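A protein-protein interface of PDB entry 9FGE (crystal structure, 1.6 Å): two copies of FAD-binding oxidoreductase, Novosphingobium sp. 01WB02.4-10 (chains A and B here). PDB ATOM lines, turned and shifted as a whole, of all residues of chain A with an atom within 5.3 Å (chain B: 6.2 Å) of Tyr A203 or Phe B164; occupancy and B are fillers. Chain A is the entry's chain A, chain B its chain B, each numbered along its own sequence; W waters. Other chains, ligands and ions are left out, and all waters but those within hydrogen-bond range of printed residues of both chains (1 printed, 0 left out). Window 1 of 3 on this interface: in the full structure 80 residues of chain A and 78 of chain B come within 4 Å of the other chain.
Phe A164 touches Tyr B203, and with the chains exchanged Tyr A203 touches Phe B164. Tyr A203 touches Gly B206, and with the chains exchanged Gly A206 touches Tyr B203. 7 positions are printed for both chains.
Tyr B203 touches Phe A164 (CD2 to CE2, 3.9 Å). Arg B153 touches Trp A198. Trp A198 touches Phe B164 (CZ3 to CD2, 3.6 Å). Met B165 touches Trp A198 (CG to CZ2, 3.7 Å). Thr B209 touches Gly A201. Pro A202 touches Gly B206 (CA to O, 3.9 Å). Pro A202 touches Thr B209. NH1 of Arg B153 touches N of Tyr A203, 3.7 Å away. CD2 of Tyr A203 touches CE2 of Phe B164 (3.9 Å). OG1 of Thr B209 touches CB of Tyr A203 (3.98 Å).
O of Phe A164 lies within hydrogen-bond range of NZ of Lys A197, 3.4 Å away. The guanidinium group (NH1) of Arg B153 lies within hydrogen-bond range of the side-chain hydroxyl (OG1) of Thr B209 (2.9 Å). The side-chain amino group of Lys B197 lies within hydrogen-bond range of the backbone carbonyl oxygen of Phe B164, at 3.4 Å. The backbone carbonyl oxygen of Met B165 sits at hydrogen-bond distance from the side-chain amino group of Lys B197, at 3.0 Å. The backbone carbonyl oxygen (O) of Gly B206 is in hydrogen-bond range of the side-chain hydroxyl (OG1) of Thr B209 (2.8 Å).
Printed residues of chain B within 4 Å of Phe A164: Tyr B203. Gln A167 touches none of the printed residues of chain B. Of the printed residues of chain B, Gly A201 touches Arg B153 and Thr B209. Printed residues of chain B within 4 Å of Pro A202: Gly B206 and Thr B209. Of the printed residues of chain B, Tyr A203 touches Arg B153 (3.7 Å), Phe B164 (3.9 Å), Gly B206 (3.0 Å), Leu B207 (3.7 Å) and Thr B209 (3.98 Å). Of the printed residues of chain B, Gly A206 touches Tyr B203 (3.0 Å). Printed residues of chain A within 4 Å of Glu B162: Trp A198. Phe B164 touches just these residues of chain A: Trp A198 (3.6 Å) and Tyr A203 (3.9 Å). The nearest printed residue of chain B that does not touch Tyr A203 is Tyr B203 (4.02 Å). The nearest printed residue of chain A that does not touch Phe B164 is Lys A197 (7.0 Å). The nearest printed residue of chain B that does not touch Phe A164 is Lys B197 (7.1 Å).
Water W1 lies within hydrogen-bond range of the backbone NH (N) of Gly B206 (2.8 Å), the backbone carbonyl oxygen (O) of Tyr B203 (2.8 Å) and the backbone carbonyl oxygen (O) of Tyr A203 (3.3 Å).
The indole nitrogen (NE1) of Trp A198 is in hydrogen-bond range of the side-chain carboxylate (OE2) of Glu B162, 2.8 Å away. The backbone carbonyl oxygen (O) of Gly A201 sits at hydrogen-bond distance from the guanidinium group (NH2) of Arg B153, at 2.8 Å. The backbone carbonyl oxygen (O) of Gly B206 sits at hydrogen-bond distance from the backbone NH (N) of Tyr A203 (3.0 Å). The backbone carbonyl oxygen (O) of Gly A206 is in hydrogen-bond range of the backbone NH (N) of Tyr B203, at 3.0 Å.
Of the 20 printed residues of chain B, 8 touch a printed residue of chain A. Hydrophobic or aromatic side chains of chain B that line the printed part of chain A: Phe B164, Met B165 and Tyr B203. Of the 10 printed residues of chain A, 6 touch a printed residue of chain B. Printed residues of chain A that touch a printed residue of chain B: Phe A164, Trp A198, Gly A201, Pro A202, Tyr A203 and Gly A206. Hydrophobic or aromatic side chains of chain A within 4 Å of the printed part of chain B: Phe A164, Trp A198 and Tyr A203.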
ATOM      1  N   PHE A 164     -22.369  14.656 -10.877  1.00  0.00           N
ATOM      2  CA  PHE A 164     -21.436  14.032  -9.965  1.00  0.00           C
ATOM      3  C   PHE A 164     -20.107  14.803  -9.888  1.00  0.00           C
ATOM      4  O   PHE A 164     -19.443  14.766  -8.844  1.00  0.00           O
ATOM      5  CB  PHE A 164     -21.287  12.536 -10.260  1.00  0.00           C
ATOM      6  CG  PHE A 164     -20.371  11.799  -9.314  1.00  0.00           C
ATOM      7  CD1 PHE A 164     -20.468  11.925  -7.935  1.00  0.00           C
ATOM      8  CD2 PHE A 164     -19.401  10.967  -9.824  1.00  0.00           C
ATOM      9  CE1 PHE A 164     -19.558  11.283  -7.092  1.00  0.00           C
ATOM     10  CE2 PHE A 164     -18.564  10.250  -8.979  1.00  0.00           C
ATOM     11  CZ  PHE A 164     -18.620  10.434  -7.615  1.00  0.00           C
ATOM     12  N   GLN A 167     -20.463  17.287  -6.894  1.00  0.00           N
ATOM     13  CA  GLN A 167     -20.670  16.768  -5.551  1.00  0.00           C
ATOM     14  C   GLN A 167     -19.394  16.921  -4.741  1.00  0.00           C
ATOM     15  O   GLN A 167     -18.287  16.715  -5.245  1.00  0.00           O
ATOM     16  CB  GLN A 167     -21.169  15.318  -5.666  1.00  0.00           C
ATOM     17  CG  GLN A 167     -21.441  14.630  -4.329  1.00  0.00           C
ATOM     18  CD  GLN A 167     -20.261  13.867  -3.776  1.00  0.00           C
ATOM     19  OE1 GLN A 167     -19.443  13.378  -4.542  1.00  0.00           O
ATOM     20  NE2 GLN A 167     -20.087  13.835  -2.473  1.00  0.00           N
ATOM     21  N   LYS A 197     -12.762  17.982  -2.566  1.00  0.00           N
ATOM     22  CA  LYS A 197     -13.486  16.735  -2.856  1.00  0.00           C
ATOM     23  C   LYS A 197     -12.833  15.488  -2.260  1.00  0.00           C
ATOM     24  O   LYS A 197     -13.540  14.568  -1.824  1.00  0.00           O
ATOM     25  CB  LYS A 197     -13.651  16.442  -4.359  1.00  0.00           C
ATOM     26  CG  LYS A 197     -14.477  17.458  -5.131  1.00  0.00           C
ATOM     27  CD  LYS A 197     -14.571  17.206  -6.626  1.00  0.00           C
ATOM     28  CE  LYS A 197     -15.077  15.839  -7.065  1.00  0.00           C
ATOM     29  NZ  LYS A 197     -16.552  15.769  -7.277  1.00  0.00           N
ATOM     30  N   TRP A 198     -11.507  15.373  -2.332  1.00  0.00           N
ATOM     31  CA  TRP A 198     -10.897  14.045  -2.324  1.00  0.00           C
ATOM     32  C   TRP A 198     -10.616  13.488  -0.929  1.00  0.00           C
ATOM     33  O   TRP A 198     -10.542  12.256  -0.762  1.00  0.00           O
ATOM     34  CB  TRP A 198      -9.555  14.065  -3.059  1.00  0.00           C
ATOM     35  CG  TRP A 198      -9.521  14.726  -4.392  1.00  0.00           C
ATOM     36  CD1 TRP A 198      -8.567  15.613  -4.799  1.00  0.00           C
ATOM     37  CD2 TRP A 198     -10.389  14.504  -5.507  1.00  0.00           C
ATOM     38  NE1 TRP A 198      -8.766  15.954  -6.078  1.00  0.00           N
ATOM     39  CE2 TRP A 198      -9.879  15.297  -6.558  1.00  0.00           C
ATOM     40  CE3 TRP A 198     -11.537  13.735  -5.725  1.00  0.00           C
ATOM     41  CZ2 TRP A 198     -10.532  15.398  -7.780  1.00  0.00           C
ATOM     42  CZ3 TRP A 198     -12.158  13.780  -6.958  1.00  0.00           C
ATOM     43  CH2 TRP A 198     -11.659  14.606  -7.971  1.00  0.00           C
ATOM     44  N   GLY A 201      -6.240   9.482   1.451  1.00  0.00           N
ATOM     45  CA  GLY A 201      -6.461   8.030   1.290  1.00  0.00           C
ATOM     46  C   GLY A 201      -7.445   7.766   0.161  1.00  0.00           C
ATOM     47  O   GLY A 201      -7.807   8.666  -0.583  1.00  0.00           O
ATOM     48  N   PRO A 202      -7.951   6.517   0.021  1.00  0.00           N
ATOM     49  CA  PRO A 202      -8.813   6.147  -1.095  1.00  0.00           C
ATOM     50  C   PRO A 202     -10.020   7.085  -1.165  1.00  0.00           C
ATOM     51  O   PRO A 202     -10.587   7.435  -0.128  1.00  0.00           O
ATOM     52  CB  PRO A 202      -9.233   4.697  -0.770  1.00  0.00           C
ATOM     53  CG  PRO A 202      -8.266   4.177   0.254  1.00  0.00           C
ATOM     54  CD  PRO A 202      -7.569   5.364   0.873  1.00  0.00           C
ATOM     55  N   TYR A 203     -10.369   7.524  -2.386  1.00  0.00           N
ATOM     56  CA  TYR A 203     -11.503   8.392  -2.645  1.00  0.00           C
ATOM     57  C   TYR A 203     -12.761   7.535  -2.724  1.00  0.00           C
ATOM     58  O   TYR A 203     -12.865   6.680  -3.618  1.00  0.00           O
ATOM     59  CB  TYR A 203     -11.329   9.127  -3.969  1.00  0.00           C
ATOM     60  CG  TYR A 203     -12.530   9.885  -4.447  1.00  0.00           C
ATOM     61  CD1 TYR A 203     -13.081  10.879  -3.686  1.00  0.00           C
ATOM     62  CD2 TYR A 203     -13.146   9.578  -5.636  1.00  0.00           C
ATOM     63  CE1 TYR A 203     -14.164  11.611  -4.112  1.00  0.00           C
ATOM     64  CE2 TYR A 203     -14.243  10.301  -6.082  1.00  0.00           C
ATOM     65  CZ  TYR A 203     -14.740  11.350  -5.332  1.00  0.00           C
ATOM     66  OH  TYR A 203     -15.821  12.064  -5.845  1.00  0.00           O
ATOM     67  N   LEU A 204     -13.671   7.720  -1.754  1.00  0.00           N
ATOM     68  CA  LEU A 204     -14.755   6.749  -1.535  1.00  0.00           C
ATOM     69  C   LEU A 204     -16.103   7.179  -2.106  1.00  0.00           C
ATOM     70  O   LEU A 204     -16.972   6.326  -2.214  1.00  0.00           O
ATOM     71  CB  LEU A 204     -14.947   6.510  -0.043  1.00  0.00           C
ATOM     72  CG  LEU A 204     -13.733   6.011   0.751  1.00  0.00           C
ATOM     73  CD1 LEU A 204     -14.082   5.849   2.213  1.00  0.00           C
ATOM     74  CD2 LEU A 204     -13.186   4.748   0.170  1.00  0.00           C
ATOM     75  N   ASP A 205     -16.336   8.451  -2.460  1.00  0.00           N
ATOM     76  CA  ASP A 205     -17.669   8.931  -2.710  1.00  0.00           C
ATOM     77  C   ASP A 205     -18.264   8.195  -3.896  1.00  0.00           C
ATOM     78  O   ASP A 205     -19.481   7.966  -3.912  1.00  0.00           O
ATOM     79  CB  ASP A 205     -17.728  10.443  -2.949  1.00  0.00           C
ATOM     80  CG  ASP A 205     -17.187  11.259  -1.792  1.00  0.00           C
ATOM     81  OD1 ASP A 205     -16.055  11.027  -1.391  1.00  0.00           O
ATOM     82  OD2 ASP A 205     -17.901  12.114  -1.291  1.00  0.00           O
ATOM     83  N   GLY A 206     -17.443   7.857  -4.886  1.00  0.00           N
ATOM     84  CA  GLY A 206     -17.953   7.148  -6.049  1.00  0.00           C
ATOM     85  C   GLY A 206     -18.536   5.752  -5.780  1.00  0.00           C
ATOM     86  O   GLY A 206     -19.401   5.255  -6.548  1.00  0.00           O
ATOM     87  N   THR B 150      -0.790  11.597 -10.614  1.00  0.00           N
ATOM     88  CA  THR B 150      -2.248  11.602 -10.608  1.00  0.00           C
ATOM     89  C   THR B 150      -2.790  10.643  -9.552  1.00  0.00           C
ATOM     90  O   THR B 150      -3.750  10.993  -8.831  1.00  0.00           O
ATOM     91  CB  THR B 150      -2.819  11.342 -12.008  1.00  0.00           C
ATOM     92  OG1 THR B 150      -2.346  12.286 -12.989  1.00  0.00           O
ATOM     93  CG2 THR B 150      -4.324  11.232 -11.966  1.00  0.00           C
ATOM     94  N   ARG B 153      -2.926  12.129  -6.344  1.00  0.00           N
ATOM     95  CA  ARG B 153      -3.787  13.295  -6.470  1.00  0.00           C
ATOM     96  C   ARG B 153      -2.999  14.596  -6.379  1.00  0.00           C
ATOM     97  O   ARG B 153      -3.415  15.562  -5.747  1.00  0.00           O
ATOM     98  CB  ARG B 153      -4.953  13.193  -5.495  1.00  0.00           C
ATOM     99  CG  ARG B 153      -5.795  11.963  -5.709  1.00  0.00           C
ATOM    100  CD  ARG B 153      -7.096  12.018  -4.954  1.00  0.00           C
ATOM    101  NE  ARG B 153      -6.918  12.045  -3.510  1.00  0.00           N
ATOM    102  CZ  ARG B 153      -7.164  11.036  -2.684  1.00  0.00           C
ATOM    103  NH1 ARG B 153      -7.550   9.852  -3.113  1.00  0.00           N
ATOM    104  NH2 ARG B 153      -7.002  11.206  -1.395  1.00  0.00           N
ATOM    105  N   GLY B 154      -1.890  14.615  -7.125  1.00  0.00           N
ATOM    106  CA  GLY B 154      -1.058  15.790  -7.296  1.00  0.00           C
ATOM    107  C   GLY B 154      -1.697  16.861  -8.159  1.00  0.00           C
ATOM    108  O   GLY B 154      -2.787  16.731  -8.720  1.00  0.00           O
ATOM    109  N   GLY B 161      -5.096  21.662 -13.784  1.00  0.00           N
ATOM    110  CA  GLY B 161      -4.156  21.482 -12.694  1.00  0.00           C
ATOM    111  C   GLY B 161      -4.590  20.460 -11.659  1.00  0.00           C
ATOM    112  O   GLY B 161      -3.705  19.903 -10.993  1.00  0.00           O
ATOM    113  N   GLU B 162      -5.895  20.295 -11.441  1.00  0.00           N
ATOM    114  CA  GLU B 162      -6.346  19.299 -10.464  1.00  0.00           C
ATOM    115  C   GLU B 162      -6.341  17.923 -11.127  1.00  0.00           C
ATOM    116  O   GLU B 162      -7.328  17.473 -11.709  1.00  0.00           O
ATOM    117  CB  GLU B 162      -7.693  19.684  -9.880  1.00  0.00           C
ATOM    118  CG  GLU B 162      -8.140  18.777  -8.754  1.00  0.00           C
ATOM    119  CD  GLU B 162      -7.282  18.801  -7.512  1.00  0.00           C
ATOM    120  OE1 GLU B 162      -6.896  19.937  -7.038  1.00  0.00           O
ATOM    121  OE2 GLU B 162      -6.883  17.724  -7.071  1.00  0.00           O
ATOM    122  N   HIS B 163      -5.154  17.267 -11.132  1.00  0.00           N
ATOM    123  CA  HIS B 163      -4.871  16.126 -11.997  1.00  0.00           C
ATOM    124  C   HIS B 163      -5.911  15.001 -11.982  1.00  0.00           C
ATOM    125  O   HIS B 163      -6.372  14.550 -13.026  1.00  0.00           O
ATOM    126  CB  HIS B 163      -3.470  15.574 -11.751  1.00  0.00           C
ATOM    127  CG  HIS B 163      -2.380  16.496 -12.067  1.00  0.00           C
ATOM    128  ND1 HIS B 163      -1.044  16.361 -11.702  1.00  0.00           N
ATOM    129  CD2 HIS B 163      -2.471  17.597 -12.862  1.00  0.00           C
ATOM    130  CE1 HIS B 163      -0.382  17.376 -12.224  1.00  0.00           C
ATOM    131  NE2 HIS B 163      -1.214  18.101 -12.963  1.00  0.00           N
ATOM    132  N   PHE B 164      -6.379  14.580 -10.816  1.00  0.00           N
ATOM    133  CA  PHE B 164      -7.312  13.459 -10.750  1.00  0.00           C
ATOM    134  C   PHE B 164      -8.646  13.824 -11.425  1.00  0.00           C
ATOM    135  O   PHE B 164      -9.338  12.938 -11.935  1.00  0.00           O
ATOM    136  CB  PHE B 164      -7.500  12.956  -9.308  1.00  0.00           C
ATOM    137  CG  PHE B 164      -8.422  11.783  -9.145  1.00  0.00           C
ATOM    138  CD1 PHE B 164      -8.337  10.666  -9.967  1.00  0.00           C
ATOM    139  CD2 PHE B 164      -9.419  11.801  -8.170  1.00  0.00           C
ATOM    140  CE1 PHE B 164      -9.257   9.619  -9.852  1.00  0.00           C
ATOM    141  CE2 PHE B 164     -10.304  10.721  -8.009  1.00  0.00           C
ATOM    142  CZ  PHE B 164     -10.215   9.635  -8.843  1.00  0.00           C
ATOM    143  N   MET B 165      -9.028  15.111 -11.507  1.00  0.00           N
ATOM    144  CA  MET B 165     -10.253  15.436 -12.211  1.00  0.00           C
ATOM    145  C   MET B 165     -10.168  15.044 -13.688  1.00  0.00           C
ATOM    146  O   MET B 165     -11.206  14.829 -14.298  1.00  0.00           O
ATOM    147  CB  MET B 165     -10.559  16.938 -12.181  1.00  0.00           C
ATOM    148  CG  MET B 165     -11.010  17.455 -10.874  1.00  0.00           C
ATOM    149  SD  MET B 165     -11.595  19.212 -10.991  1.00  0.00           S
ATOM    150  CE  MET B 165     -12.158  19.590  -9.321  1.00  0.00           C
ATOM    151  N   PHE B 166      -8.972  15.011 -14.270  1.00  0.00           N
ATOM    152  CA  PHE B 166      -8.786  14.831 -15.703  1.00  0.00           C
ATOM    153  C   PHE B 166      -8.371  13.409 -16.060  1.00  0.00           C
ATOM    154  O   PHE B 166      -8.129  13.089 -17.215  1.00  0.00           O
ATOM    155  CB  PHE B 166      -7.767  15.890 -16.195  1.00  0.00           C
ATOM    156  CG  PHE B 166      -8.296  17.272 -15.996  1.00  0.00           C
ATOM    157  CD1 PHE B 166      -9.171  17.831 -16.933  1.00  0.00           C
ATOM    158  CD2 PHE B 166      -8.040  17.991 -14.826  1.00  0.00           C
ATOM    159  CE1 PHE B 166      -9.780  19.056 -16.702  1.00  0.00           C
ATOM    160  CE2 PHE B 166      -8.708  19.193 -14.593  1.00  0.00           C
ATOM    161  CZ  PHE B 166      -9.538  19.730 -15.540  1.00  0.00           C
ATOM    162  N   GLN B 167      -8.277  12.517 -15.065  1.00  0.00           N
ATOM    163  CA  GLN B 167      -8.076  11.109 -15.328  1.00  0.00           C
ATOM    164  C   GLN B 167      -9.352  10.508 -15.906  1.00  0.00           C
ATOM    165  O   GLN B 167     -10.455  10.843 -15.483  1.00  0.00           O
ATOM    166  CB  GLN B 167      -7.675  10.441 -13.997  1.00  0.00           C
ATOM    167  CG  GLN B 167      -7.438   8.954 -14.088  1.00  0.00           C
ATOM    168  CD  GLN B 167      -8.632   8.120 -13.700  1.00  0.00           C
ATOM    169  OE1 GLN B 167      -9.433   8.518 -12.866  1.00  0.00           O
ATOM    170  NE2 GLN B 167      -8.768   6.987 -14.315  1.00  0.00           N
ATOM    171  N   CYS B 168      -9.221   9.579 -16.827  1.00  0.00           N
ATOM    172  CA  CYS B 168     -10.362   8.927 -17.462  1.00  0.00           C
ATOM    173  C   CYS B 168     -10.005   7.533 -17.962  1.00  0.00           C
ATOM    174  O   CYS B 168      -9.315   7.402 -18.965  1.00  0.00           O
ATOM    175  CB  CYS B 168     -10.889   9.776 -18.626  1.00  0.00           C
ATOM    176  SG  CYS B 168     -12.540   9.279 -19.226  1.00  0.00           S
ATOM    177  N   MET B 170      -8.814   3.539 -16.296  1.00  0.00           N
ATOM    178  CA  MET B 170      -7.554   2.958 -15.880  1.00  0.00           C
ATOM    179  C   MET B 170      -7.660   1.429 -16.009  1.00  0.00           C
ATOM    180  O   MET B 170      -8.741   0.826 -15.980  1.00  0.00           O
ATOM    181  CB  MET B 170      -7.138   3.388 -14.473  1.00  0.00           C
ATOM    182  CG  MET B 170      -8.077   2.951 -13.402  1.00  0.00           C
ATOM    183  SD  MET B 170      -7.436   3.257 -11.741  1.00  0.00           S
ATOM    184  CE  MET B 170      -7.151   5.004 -11.652  1.00  0.00           C
ATOM    185  N   LYS B 197     -16.017   9.218 -17.930  1.00  0.00           N
ATOM    186  CA  LYS B 197     -15.289   8.797 -16.745  1.00  0.00           C
ATOM    187  C   LYS B 197     -15.973   7.675 -15.973  1.00  0.00           C
ATOM    188  O   LYS B 197     -15.317   6.827 -15.377  1.00  0.00           O
ATOM    189  CB  LYS B 197     -15.084   9.959 -15.778  1.00  0.00           C
ATOM    190  CG  LYS B 197     -14.081  11.025 -16.145  1.00  0.00           C
ATOM    191  CD  LYS B 197     -14.156  12.275 -15.273  1.00  0.00           C
ATOM    192  CE  LYS B 197     -13.678  12.079 -13.839  1.00  0.00           C
ATOM    193  NZ  LYS B 197     -12.184  12.085 -13.665  1.00  0.00           N
ATOM    194  N   TYR B 203     -18.543   3.829  -9.000  1.00  0.00           N
ATOM    195  CA  TYR B 203     -17.377   4.442  -9.603  1.00  0.00           C
ATOM    196  C   TYR B 203     -16.146   4.053  -8.793  1.00  0.00           C
ATOM    197  O   TYR B 203     -16.060   4.425  -7.624  1.00  0.00           O
ATOM    198  CB  TYR B 203     -17.578   5.946  -9.661  1.00  0.00           C
ATOM    199  CG  TYR B 203     -16.343   6.711 -10.065  1.00  0.00           C
ATOM    200  CD1 TYR B 203     -15.795   6.576 -11.318  1.00  0.00           C
ATOM    201  CD2 TYR B 203     -15.725   7.565  -9.186  1.00  0.00           C
ATOM    202  CE1 TYR B 203     -14.693   7.320 -11.699  1.00  0.00           C
ATOM    203  CE2 TYR B 203     -14.613   8.317  -9.554  1.00  0.00           C
ATOM    204  CZ  TYR B 203     -14.134   8.223 -10.830  1.00  0.00           C
ATOM    205  OH  TYR B 203     -13.042   9.022 -11.107  1.00  0.00           O
ATOM    206  N   LEU B 204     -15.213   3.356  -9.438  1.00  0.00           N
ATOM    207  CA  LEU B 204     -14.148   2.631  -8.745  1.00  0.00           C
ATOM    208  C   LEU B 204     -12.785   3.336  -8.832  1.00  0.00           C
ATOM    209  O   LEU B 204     -11.930   3.003  -8.032  1.00  0.00           O
ATOM    210  CB  LEU B 204     -13.987   1.203  -9.305  1.00  0.00           C
ATOM    211  CG  LEU B 204     -15.242   0.291  -9.329  1.00  0.00           C
ATOM    212  CD1 LEU B 204     -14.951  -1.053  -9.942  1.00  0.00           C
ATOM    213  CD2 LEU B 204     -15.792   0.135  -7.951  1.00  0.00           C
ATOM    214  N   ASP B 205     -12.537   4.243  -9.796  1.00  0.00           N
ATOM    215  CA  ASP B 205     -11.172   4.723 -10.065  1.00  0.00           C
ATOM    216  C   ASP B 205     -10.577   5.326  -8.783  1.00  0.00           C
ATOM    217  O   ASP B 205      -9.373   5.224  -8.556  1.00  0.00           O
ATOM    218  CB  ASP B 205     -11.142   5.695 -11.248  1.00  0.00           C
ATOM    219  CG  ASP B 205     -11.733   5.121 -12.527  1.00  0.00           C
ATOM    220  OD1 ASP B 205     -12.903   4.594 -12.455  1.00  0.00           O
ATOM    221  OD2 ASP B 205     -10.990   5.125 -13.544  1.00  0.00           O
ATOM    222  N   GLY B 206     -11.406   6.023  -7.986  1.00  0.00           N
ATOM    223  CA  GLY B 206     -10.890   6.659  -6.786  1.00  0.00           C
ATOM    224  C   GLY B 206     -10.347   5.711  -5.716  1.00  0.00           C
ATOM    225  O   GLY B 206      -9.504   6.105  -4.889  1.00  0.00           O
ATOM    226  N   LEU B 207     -10.809   4.456  -5.723  1.00  0.00           N
ATOM    227  CA  LEU B 207     -10.285   3.438  -4.838  1.00  0.00           C
ATOM    228  C   LEU B 207      -8.812   3.186  -5.075  1.00  0.00           C
ATOM    229  O   LEU B 207      -8.160   2.587  -4.221  1.00  0.00           O
ATOM    230  CB  LEU B 207     -10.962   2.075  -5.045  1.00  0.00           C
ATOM    231  CG  LEU B 207     -12.357   1.917  -4.488  1.00  0.00           C
ATOM    232  CD1 LEU B 207     -12.789   0.499  -4.735  1.00  0.00           C
ATOM    233  CD2 LEU B 207     -12.385   2.261  -3.001  1.00  0.00           C
ATOM    234  N   PHE B 208      -8.301   3.509  -6.274  1.00  0.00           N
ATOM    235  CA  PHE B 208      -6.917   3.221  -6.617  1.00  0.00           C
ATOM    236  C   PHE B 208      -6.043   4.479  -6.540  1.00  0.00           C
ATOM    237  O   PHE B 208      -4.930   4.471  -7.093  1.00  0.00           O
ATOM    238  CB  PHE B 208      -6.856   2.535  -8.006  1.00  0.00           C
ATOM    239  CG  PHE B 208      -7.703   1.282  -8.027  1.00  0.00           C
ATOM    240  CD1 PHE B 208      -7.304   0.191  -7.291  1.00  0.00           C
ATOM    241  CD2 PHE B 208      -8.947   1.227  -8.648  1.00  0.00           C
ATOM    242  CE1 PHE B 208      -8.088  -0.953  -7.260  1.00  0.00           C
ATOM    243  CE2 PHE B 208      -9.728   0.083  -8.608  1.00  0.00           C
ATOM    244  CZ  PHE B 208      -9.287  -1.004  -7.901  1.00  0.00           C
ATOM    245  N   THR B 209      -6.549   5.549  -5.882  1.00  0.00           N
ATOM    246  CA  THR B 209      -5.803   6.753  -5.629  1.00  0.00           C
ATOM    247  C   THR B 209      -5.508   6.828  -4.146  1.00  0.00           C
ATOM    248  O   THR B 209      -6.346   6.447  -3.286  1.00  0.00           O
ATOM    249  CB  THR B 209      -6.531   7.993  -6.173  1.00  0.00           C
ATOM    250  OG1 THR B 209      -7.761   8.220  -5.472  1.00  0.00           O
ATOM    251  CG2 THR B 209      -6.784   7.891  -7.654  1.00  0.00           C
HETATM  252  O   HOH W   1     -13.857   5.901  -6.713  1.00  0.00           O
